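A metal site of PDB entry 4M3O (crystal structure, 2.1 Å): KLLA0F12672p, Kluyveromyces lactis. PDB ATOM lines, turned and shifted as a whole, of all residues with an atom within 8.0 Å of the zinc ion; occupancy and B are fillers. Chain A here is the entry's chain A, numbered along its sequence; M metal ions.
Within 4 Å of the zinc ion: Cys 74, Cys 79, Cys 112 and His 116. The nearest printed residue that does not touch the zinc ion is Tyr 76 (4.8 Å).
ND1 of His 116 is bound to the zinc ion, 2.2 Å away. The side-chain sulfur (SG) of Cys 112 binds the zinc ion (2.3 Å). SG of Cys 79 binds the zinc ion, at 2.3 Å. The zinc ion is bound by SG of Cys 74. The zinc ion has four donor atoms within binding distance.
The backbone NH of Cys 74 is in hydrogen-bond range of the backbone carbonyl oxygen of Lys 81, at 2.6 Å. The backbone carbonyl oxygen of Cys 74 is in hydrogen-bond range of the guanidinium group of Arg 68, 2.9 Å away. OG1 of Thr 113 lies close to SG of Cys 112 (3.5 Å). The backbone NH (N) of His 116 is in hydrogen-bond range of the side-chain hydroxyl (OG1) of Thr 113, 3.1 Å away. The guanidinium group of Arg 68 sits at hydrogen-bond distance from the backbone carbonyl oxygen of Cys 79 (2.9 Å). The side-chain carboxylate of Glu 154 sits at hydrogen-bond distance from a ring nitrogen (NE2) of His 116, at 2.8 Å. SG of Cys 74 lies close to N of Tyr 76 (3.6 Å). N of Lys 81 sits close to SG of Cys 79, at 3.4 Å.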
ATOM      1  N   ARG A  68      20.821   4.804  -2.564  1.00  0.00           N
ATOM      2  CA  ARG A  68      20.049   5.801  -3.320  1.00  0.00           C
ATOM      3  C   ARG A  68      19.580   5.258  -4.677  1.00  0.00           C
ATOM      4  O   ARG A  68      18.417   5.496  -5.127  1.00  0.00           O
ATOM      5  CB  ARG A  68      20.819   7.114  -3.508  1.00  0.00           C
ATOM      6  CG  ARG A  68      20.815   8.038  -2.276  1.00  0.00           C
ATOM      7  CD  ARG A  68      21.715   9.229  -2.470  1.00  0.00           C
ATOM      8  NE  ARG A  68      21.337  10.090  -3.579  1.00  0.00           N
ATOM      9  CZ  ARG A  68      20.433  11.055  -3.470  1.00  0.00           C
ATOM     10  NH1 ARG A  68      19.807  11.255  -2.298  1.00  0.00           N
ATOM     11  NH2 ARG A  68      20.136  11.819  -4.545  1.00  0.00           N
ATOM     12  N   ARG A  73      17.270   6.914  -7.108  1.00  0.00           N
ATOM     13  CA  ARG A  73      17.878   8.286  -7.120  1.00  0.00           C
ATOM     14  C   ARG A  73      19.289   8.249  -7.642  1.00  0.00           C
ATOM     15  O   ARG A  73      20.077   7.269  -7.354  1.00  0.00           O
ATOM     16  CB  ARG A  73      17.756   8.890  -5.737  1.00  0.00           C
ATOM     17  CG  ARG A  73      16.310   9.338  -5.491  1.00  0.00           C
ATOM     18  CD  ARG A  73      15.822   9.158  -4.079  1.00  0.00           C
ATOM     19  NE  ARG A  73      15.842  10.442  -3.396  1.00  0.00           N
ATOM     20  CZ  ARG A  73      14.826  11.017  -2.777  1.00  0.00           C
ATOM     21  NH1 ARG A  73      13.643  10.441  -2.642  1.00  0.00           N
ATOM     22  NH2 ARG A  73      15.036  12.192  -2.211  1.00  0.00           N
ATOM     23  N   CYS A  74      19.602   9.238  -8.476  1.00  0.00           N
ATOM     24  CA  CYS A  74      21.003   9.531  -8.806  1.00  0.00           C
ATOM     25  C   CYS A  74      21.850   9.433  -7.533  1.00  0.00           C
ATOM     26  O   CYS A  74      21.450   9.882  -6.439  1.00  0.00           O
ATOM     27  CB  CYS A  74      21.166  10.905  -9.439  1.00  0.00           C
ATOM     28  SG  CYS A  74      22.907  11.338  -9.860  1.00  0.00           S
ATOM     29  N   GLY A  75      23.003   8.803  -7.688  1.00  0.00           N
ATOM     30  CA  GLY A  75      23.932   8.595  -6.601  1.00  0.00           C
ATOM     31  C   GLY A  75      24.399   9.850  -5.907  1.00  0.00           C
ATOM     32  O   GLY A  75      24.561   9.868  -4.687  1.00  0.00           O
ATOM     33  N   TYR A  76      24.573  10.901  -6.672  1.00  0.00           N
ATOM     34  CA  TYR A  76      25.056  12.202  -6.124  1.00  0.00           C
ATOM     35  C   TYR A  76      23.966  12.868  -5.291  1.00  0.00           C
ATOM     36  O   TYR A  76      22.906  13.187  -5.819  1.00  0.00           O
ATOM     37  CB  TYR A  76      25.555  13.126  -7.231  1.00  0.00           C
ATOM     38  CG  TYR A  76      26.366  14.350  -6.812  1.00  0.00           C
ATOM     39  CD1 TYR A  76      27.449  14.232  -5.934  1.00  0.00           C
ATOM     40  CD2 TYR A  76      26.069  15.630  -7.335  1.00  0.00           C
ATOM     41  CE1 TYR A  76      28.231  15.313  -5.600  1.00  0.00           C
ATOM     42  CE2 TYR A  76      26.844  16.757  -7.010  1.00  0.00           C
ATOM     43  CZ  TYR A  76      27.887  16.594  -6.121  1.00  0.00           C
ATOM     44  OH  TYR A  76      28.703  17.638  -5.773  1.00  0.00           O
ATOM     45  N   PRO A  77      24.187  12.970  -3.962  1.00  0.00           N
ATOM     46  CA  PRO A  77      23.147  13.358  -3.002  1.00  0.00           C
ATOM     47  C   PRO A  77      22.445  14.718  -3.262  1.00  0.00           C
ATOM     48  O   PRO A  77      21.322  14.868  -2.904  1.00  0.00           O
ATOM     49  CB  PRO A  77      23.877  13.344  -1.618  1.00  0.00           C
ATOM     50  CG  PRO A  77      25.098  12.544  -1.832  1.00  0.00           C
ATOM     51  CD  PRO A  77      25.438  12.566  -3.289  1.00  0.00           C
ATOM     52  N   LEU A  78      23.107  15.657  -3.924  1.00  0.00           N
ATOM     53  CA  LEU A  78      22.486  16.930  -4.332  1.00  0.00           C
ATOM     54  C   LEU A  78      21.469  16.819  -5.470  1.00  0.00           C
ATOM     55  O   LEU A  78      20.775  17.768  -5.744  1.00  0.00           O
ATOM     56  CB  LEU A  78      23.529  17.896  -4.788  1.00  0.00           C
ATOM     57  CG  LEU A  78      24.440  18.479  -3.709  1.00  0.00           C
ATOM     58  CD1 LEU A  78      25.613  19.094  -4.438  1.00  0.00           C
ATOM     59  CD2 LEU A  78      23.684  19.551  -2.900  1.00  0.00           C
ATOM     60  N   CYS A  79      21.382  15.661  -6.094  1.00  0.00           N
ATOM     61  CA  CYS A  79      20.550  15.499  -7.285  1.00  0.00           C
ATOM     62  C   CYS A  79      19.182  14.938  -6.936  1.00  0.00           C
ATOM     63  O   CYS A  79      19.074  14.018  -6.097  1.00  0.00           O
ATOM     64  CB  CYS A  79      21.214  14.493  -8.199  1.00  0.00           C
ATOM     65  SG  CYS A  79      20.568  14.427  -9.888  1.00  0.00           S
ATOM     66  N   SER A  80      18.164  15.396  -7.636  1.00  0.00           N
ATOM     67  CA  SER A  80      16.816  14.875  -7.438  1.00  0.00           C
ATOM     68  C   SER A  80      16.327  14.133  -8.691  1.00  0.00           C
ATOM     69  O   SER A  80      15.158  13.873  -8.822  1.00  0.00           O
ATOM     70  CB  SER A  80      15.860  16.027  -7.096  1.00  0.00           C
ATOM     71  OG  SER A  80      15.869  16.970  -8.146  1.00  0.00           O
ATOM     72  N   LYS A  81      17.230  13.787  -9.590  1.00  0.00           N
ATOM     73  CA  LYS A  81      16.879  12.824 -10.657  1.00  0.00           C
ATOM     74  C   LYS A  81      17.253  11.394 -10.294  1.00  0.00           C
ATOM     75  O   LYS A  81      17.910  11.121  -9.259  1.00  0.00           O
ATOM     76  CB  LYS A  81      17.563  13.218 -11.956  1.00  0.00           C
ATOM     77  CG  LYS A  81      17.318  14.676 -12.250  1.00  0.00           C
ATOM     78  CD  LYS A  81      17.962  15.146 -13.532  1.00  0.00           C
ATOM     79  CE  LYS A  81      17.963  16.656 -13.537  1.00  0.00           C
ATOM     80  NZ  LYS A  81      17.899  17.164 -14.913  1.00  0.00           N
ATOM     81  N   SER A  82      16.856  10.465 -11.177  1.00  0.00           N
ATOM     82  CA  SER A  82      17.255   9.047 -11.151  1.00  0.00           C
ATOM     83  C   SER A  82      18.533   8.850 -11.875  1.00  0.00           C
ATOM     84  O   SER A  82      18.852   9.651 -12.769  1.00  0.00           O
ATOM     85  CB  SER A  82      16.238   8.221 -11.910  1.00  0.00           C
ATOM     86  OG  SER A  82      15.019   8.347 -11.265  1.00  0.00           O
ATOM     87  N   GLN A  83      19.185   7.737 -11.621  1.00  0.00           N
ATOM     88  CA  GLN A  83      20.251   7.316 -12.474  1.00  0.00           C
ATOM     89  C   GLN A  83      19.676   7.205 -13.859  1.00  0.00           C
ATOM     90  O   GLN A  83      18.505   7.050 -14.014  1.00  0.00           O
ATOM     91  CB  GLN A  83      20.825   5.997 -11.990  1.00  0.00           C
ATOM     92  CG  GLN A  83      19.833   4.859 -11.921  1.00  0.00           C
ATOM     93  CD  GLN A  83      19.162   4.717 -10.574  1.00  0.00           C
ATOM     94  OE1 GLN A  83      18.586   5.635 -10.072  1.00  0.00           O
ATOM     95  NE2 GLN A  83      19.245   3.551 -10.009  1.00  0.00           N
ATOM     96  N   ALA A  84      20.490   7.315 -14.868  1.00  0.00           N
ATOM     97  CA  ALA A  84      19.977   7.345 -16.245  1.00  0.00           C
ATOM     98  C   ALA A  84      19.446   5.978 -16.679  1.00  0.00           C
ATOM     99  O   ALA A  84      18.451   5.922 -17.393  1.00  0.00           O
ATOM    100  CB  ALA A  84      21.056   7.809 -17.196  1.00  0.00           C
ATOM    101  N   GLU A 110      24.438   4.354 -12.076  1.00  0.00           N
ATOM    102  CA  GLU A 110      24.524   4.956 -10.756  1.00  0.00           C
ATOM    103  C   GLU A 110      24.259   6.486 -10.709  1.00  0.00           C
ATOM    104  O   GLU A 110      23.857   7.037  -9.669  1.00  0.00           O
ATOM    105  CB  GLU A 110      25.912   4.668 -10.198  1.00  0.00           C
ATOM    106  CG  GLU A 110      26.202   3.195 -10.009  1.00  0.00           C
ATOM    107  CD  GLU A 110      27.598   2.937  -9.465  1.00  0.00           C
ATOM    108  OE1 GLU A 110      28.444   3.863  -9.396  1.00  0.00           O
ATOM    109  OE2 GLU A 110      27.861   1.789  -9.141  1.00  0.00           O
ATOM    110  N   TYR A 111      24.399   7.146 -11.841  1.00  0.00           N
ATOM    111  CA  TYR A 111      24.249   8.585 -11.948  1.00  0.00           C
ATOM    112  C   TYR A 111      23.388   8.922 -13.109  1.00  0.00           C
ATOM    113  O   TYR A 111      23.339   8.164 -14.067  1.00  0.00           O
ATOM    114  CB  TYR A 111      25.658   9.216 -12.116  1.00  0.00           C
ATOM    115  CG  TYR A 111      26.474   8.884 -10.939  1.00  0.00           C
ATOM    116  CD1 TYR A 111      27.391   7.833 -10.971  1.00  0.00           C
ATOM    117  CD2 TYR A 111      26.293   9.603  -9.751  1.00  0.00           C
ATOM    118  CE1 TYR A 111      28.114   7.497  -9.818  1.00  0.00           C
ATOM    119  CE2 TYR A 111      27.034   9.288  -8.610  1.00  0.00           C
ATOM    120  CZ  TYR A 111      27.938   8.232  -8.645  1.00  0.00           C
ATOM    121  OH  TYR A 111      28.612   7.885  -7.461  1.00  0.00           O
ATOM    122  N   CYS A 112      22.806  10.129 -13.074  1.00  0.00           N
ATOM    123  CA  CYS A 112      21.995  10.678 -14.150  1.00  0.00           C
ATOM    124  C   CYS A 112      22.831  11.017 -15.386  1.00  0.00           C
ATOM    125  O   CYS A 112      22.355  10.878 -16.519  1.00  0.00           O
ATOM    126  CB  CYS A 112      21.223  11.951 -13.695  1.00  0.00           C
ATOM    127  SG  CYS A 112      22.288  13.327 -13.152  1.00  0.00           S
ATOM    128  N   THR A 113      24.093  11.400 -15.153  1.00  0.00           N
ATOM    129  CA  THR A 113      25.003  11.970 -16.208  1.00  0.00           C
ATOM    130  C   THR A 113      26.478  11.688 -15.905  1.00  0.00           C
ATOM    131  O   THR A 113      26.821  11.294 -14.783  1.00  0.00           O
ATOM    132  CB  THR A 113      24.925  13.539 -16.234  1.00  0.00           C
ATOM    133  OG1 THR A 113      25.185  14.061 -14.906  1.00  0.00           O
ATOM    134  CG2 THR A 113      23.554  13.982 -16.677  1.00  0.00           C
ATOM    135  N   LYS A 114      27.359  11.961 -16.861  1.00  0.00           N
ATOM    136  CA  LYS A 114      28.788  11.754 -16.577  1.00  0.00           C
ATOM    137  C   LYS A 114      29.309  12.835 -15.572  1.00  0.00           C
ATOM    138  O   LYS A 114      30.247  12.605 -14.757  1.00  0.00           O
ATOM    139  CB  LYS A 114      29.565  11.829 -17.875  1.00  0.00           C
ATOM    140  CG  LYS A 114      31.019  11.402 -17.751  1.00  0.00           C
ATOM    141  CD  LYS A 114      31.860  12.273 -18.651  1.00  0.00           C
ATOM    142  CE  LYS A 114      31.996  13.682 -18.075  1.00  0.00           C
ATOM    143  NZ  LYS A 114      33.138  14.394 -18.687  1.00  0.00           N
ATOM    144  N   ALA A 115      28.698  13.983 -15.655  1.00  0.00           N
ATOM    145  CA  ALA A 115      29.019  15.132 -14.864  1.00  0.00           C
ATOM    146  C   ALA A 115      28.821  14.766 -13.374  1.00  0.00           C
ATOM    147  O   ALA A 115      29.736  14.984 -12.534  1.00  0.00           O
ATOM    148  CB  ALA A 115      28.138  16.313 -15.302  1.00  0.00           C
ATOM    149  N   HIS A 116      27.679  14.139 -13.067  1.00  0.00           N
ATOM    150  CA  HIS A 116      27.362  13.719 -11.676  1.00  0.00           C
ATOM    151  C   HIS A 116      28.192  12.545 -11.230  1.00  0.00           C
ATOM    152  O   HIS A 116      28.596  12.503 -10.065  1.00  0.00           O
ATOM    153  CB  HIS A 116      25.852  13.572 -11.441  1.00  0.00           C
ATOM    154  CG  HIS A 116      25.191  14.874 -11.115  1.00  0.00           C
ATOM    155  ND1 HIS A 116      23.867  14.993 -10.768  1.00  0.00           N
ATOM    156  CD2 HIS A 116      25.709  16.120 -11.003  1.00  0.00           C
ATOM    157  CE1 HIS A 116      23.587  16.257 -10.499  1.00  0.00           C
ATOM    158  NE2 HIS A 116      24.688  16.968 -10.628  1.00  0.00           N
ATOM    159  N   PHE A 117      28.505  11.616 -12.149  1.00  0.00           N
ATOM    160  CA  PHE A 117      29.616  10.686 -11.907  1.00  0.00           C
ATOM    161  C   PHE A 117      30.927  11.400 -11.412  1.00  0.00           C
ATOM    162  O   PHE A 117      31.466  11.027 -10.404  1.00  0.00           O
ATOM    163  CB  PHE A 117      29.902   9.829 -13.167  1.00  0.00           C
ATOM    164  CG  PHE A 117      31.075   8.925 -13.034  1.00  0.00           C
ATOM    165  CD1 PHE A 117      31.242   8.108 -11.949  1.00  0.00           C
ATOM    166  CD2 PHE A 117      32.029   8.882 -14.039  1.00  0.00           C
ATOM    167  CE1 PHE A 117      32.334   7.258 -11.850  1.00  0.00           C
ATOM    168  CE2 PHE A 117      33.118   8.061 -13.944  1.00  0.00           C
ATOM    169  CZ  PHE A 117      33.273   7.228 -12.880  1.00  0.00           C
ATOM    170  N   GLU A 154      29.037  21.547 -11.700  1.00  0.00           N
ATOM    171  CA  GLU A 154      28.597  20.655 -12.758  1.00  0.00           C
ATOM    172  C   GLU A 154      29.097  21.090 -14.094  1.00  0.00           C
ATOM    173  O   GLU A 154      29.552  20.255 -14.912  1.00  0.00           O
ATOM    174  CB  GLU A 154      27.065  20.654 -12.930  1.00  0.00           C
ATOM    175  CG  GLU A 154      26.340  19.637 -12.100  1.00  0.00           C
ATOM    176  CD  GLU A 154      25.677  20.271 -10.894  1.00  0.00           C
ATOM    177  OE1 GLU A 154      26.232  21.315 -10.448  1.00  0.00           O
ATOM    178  OE2 GLU A 154      24.617  19.739 -10.425  1.00  0.00           O
HETATM  179 ZN    ZN M   1      22.352  13.346 -10.864  1.00  0.00          ZN
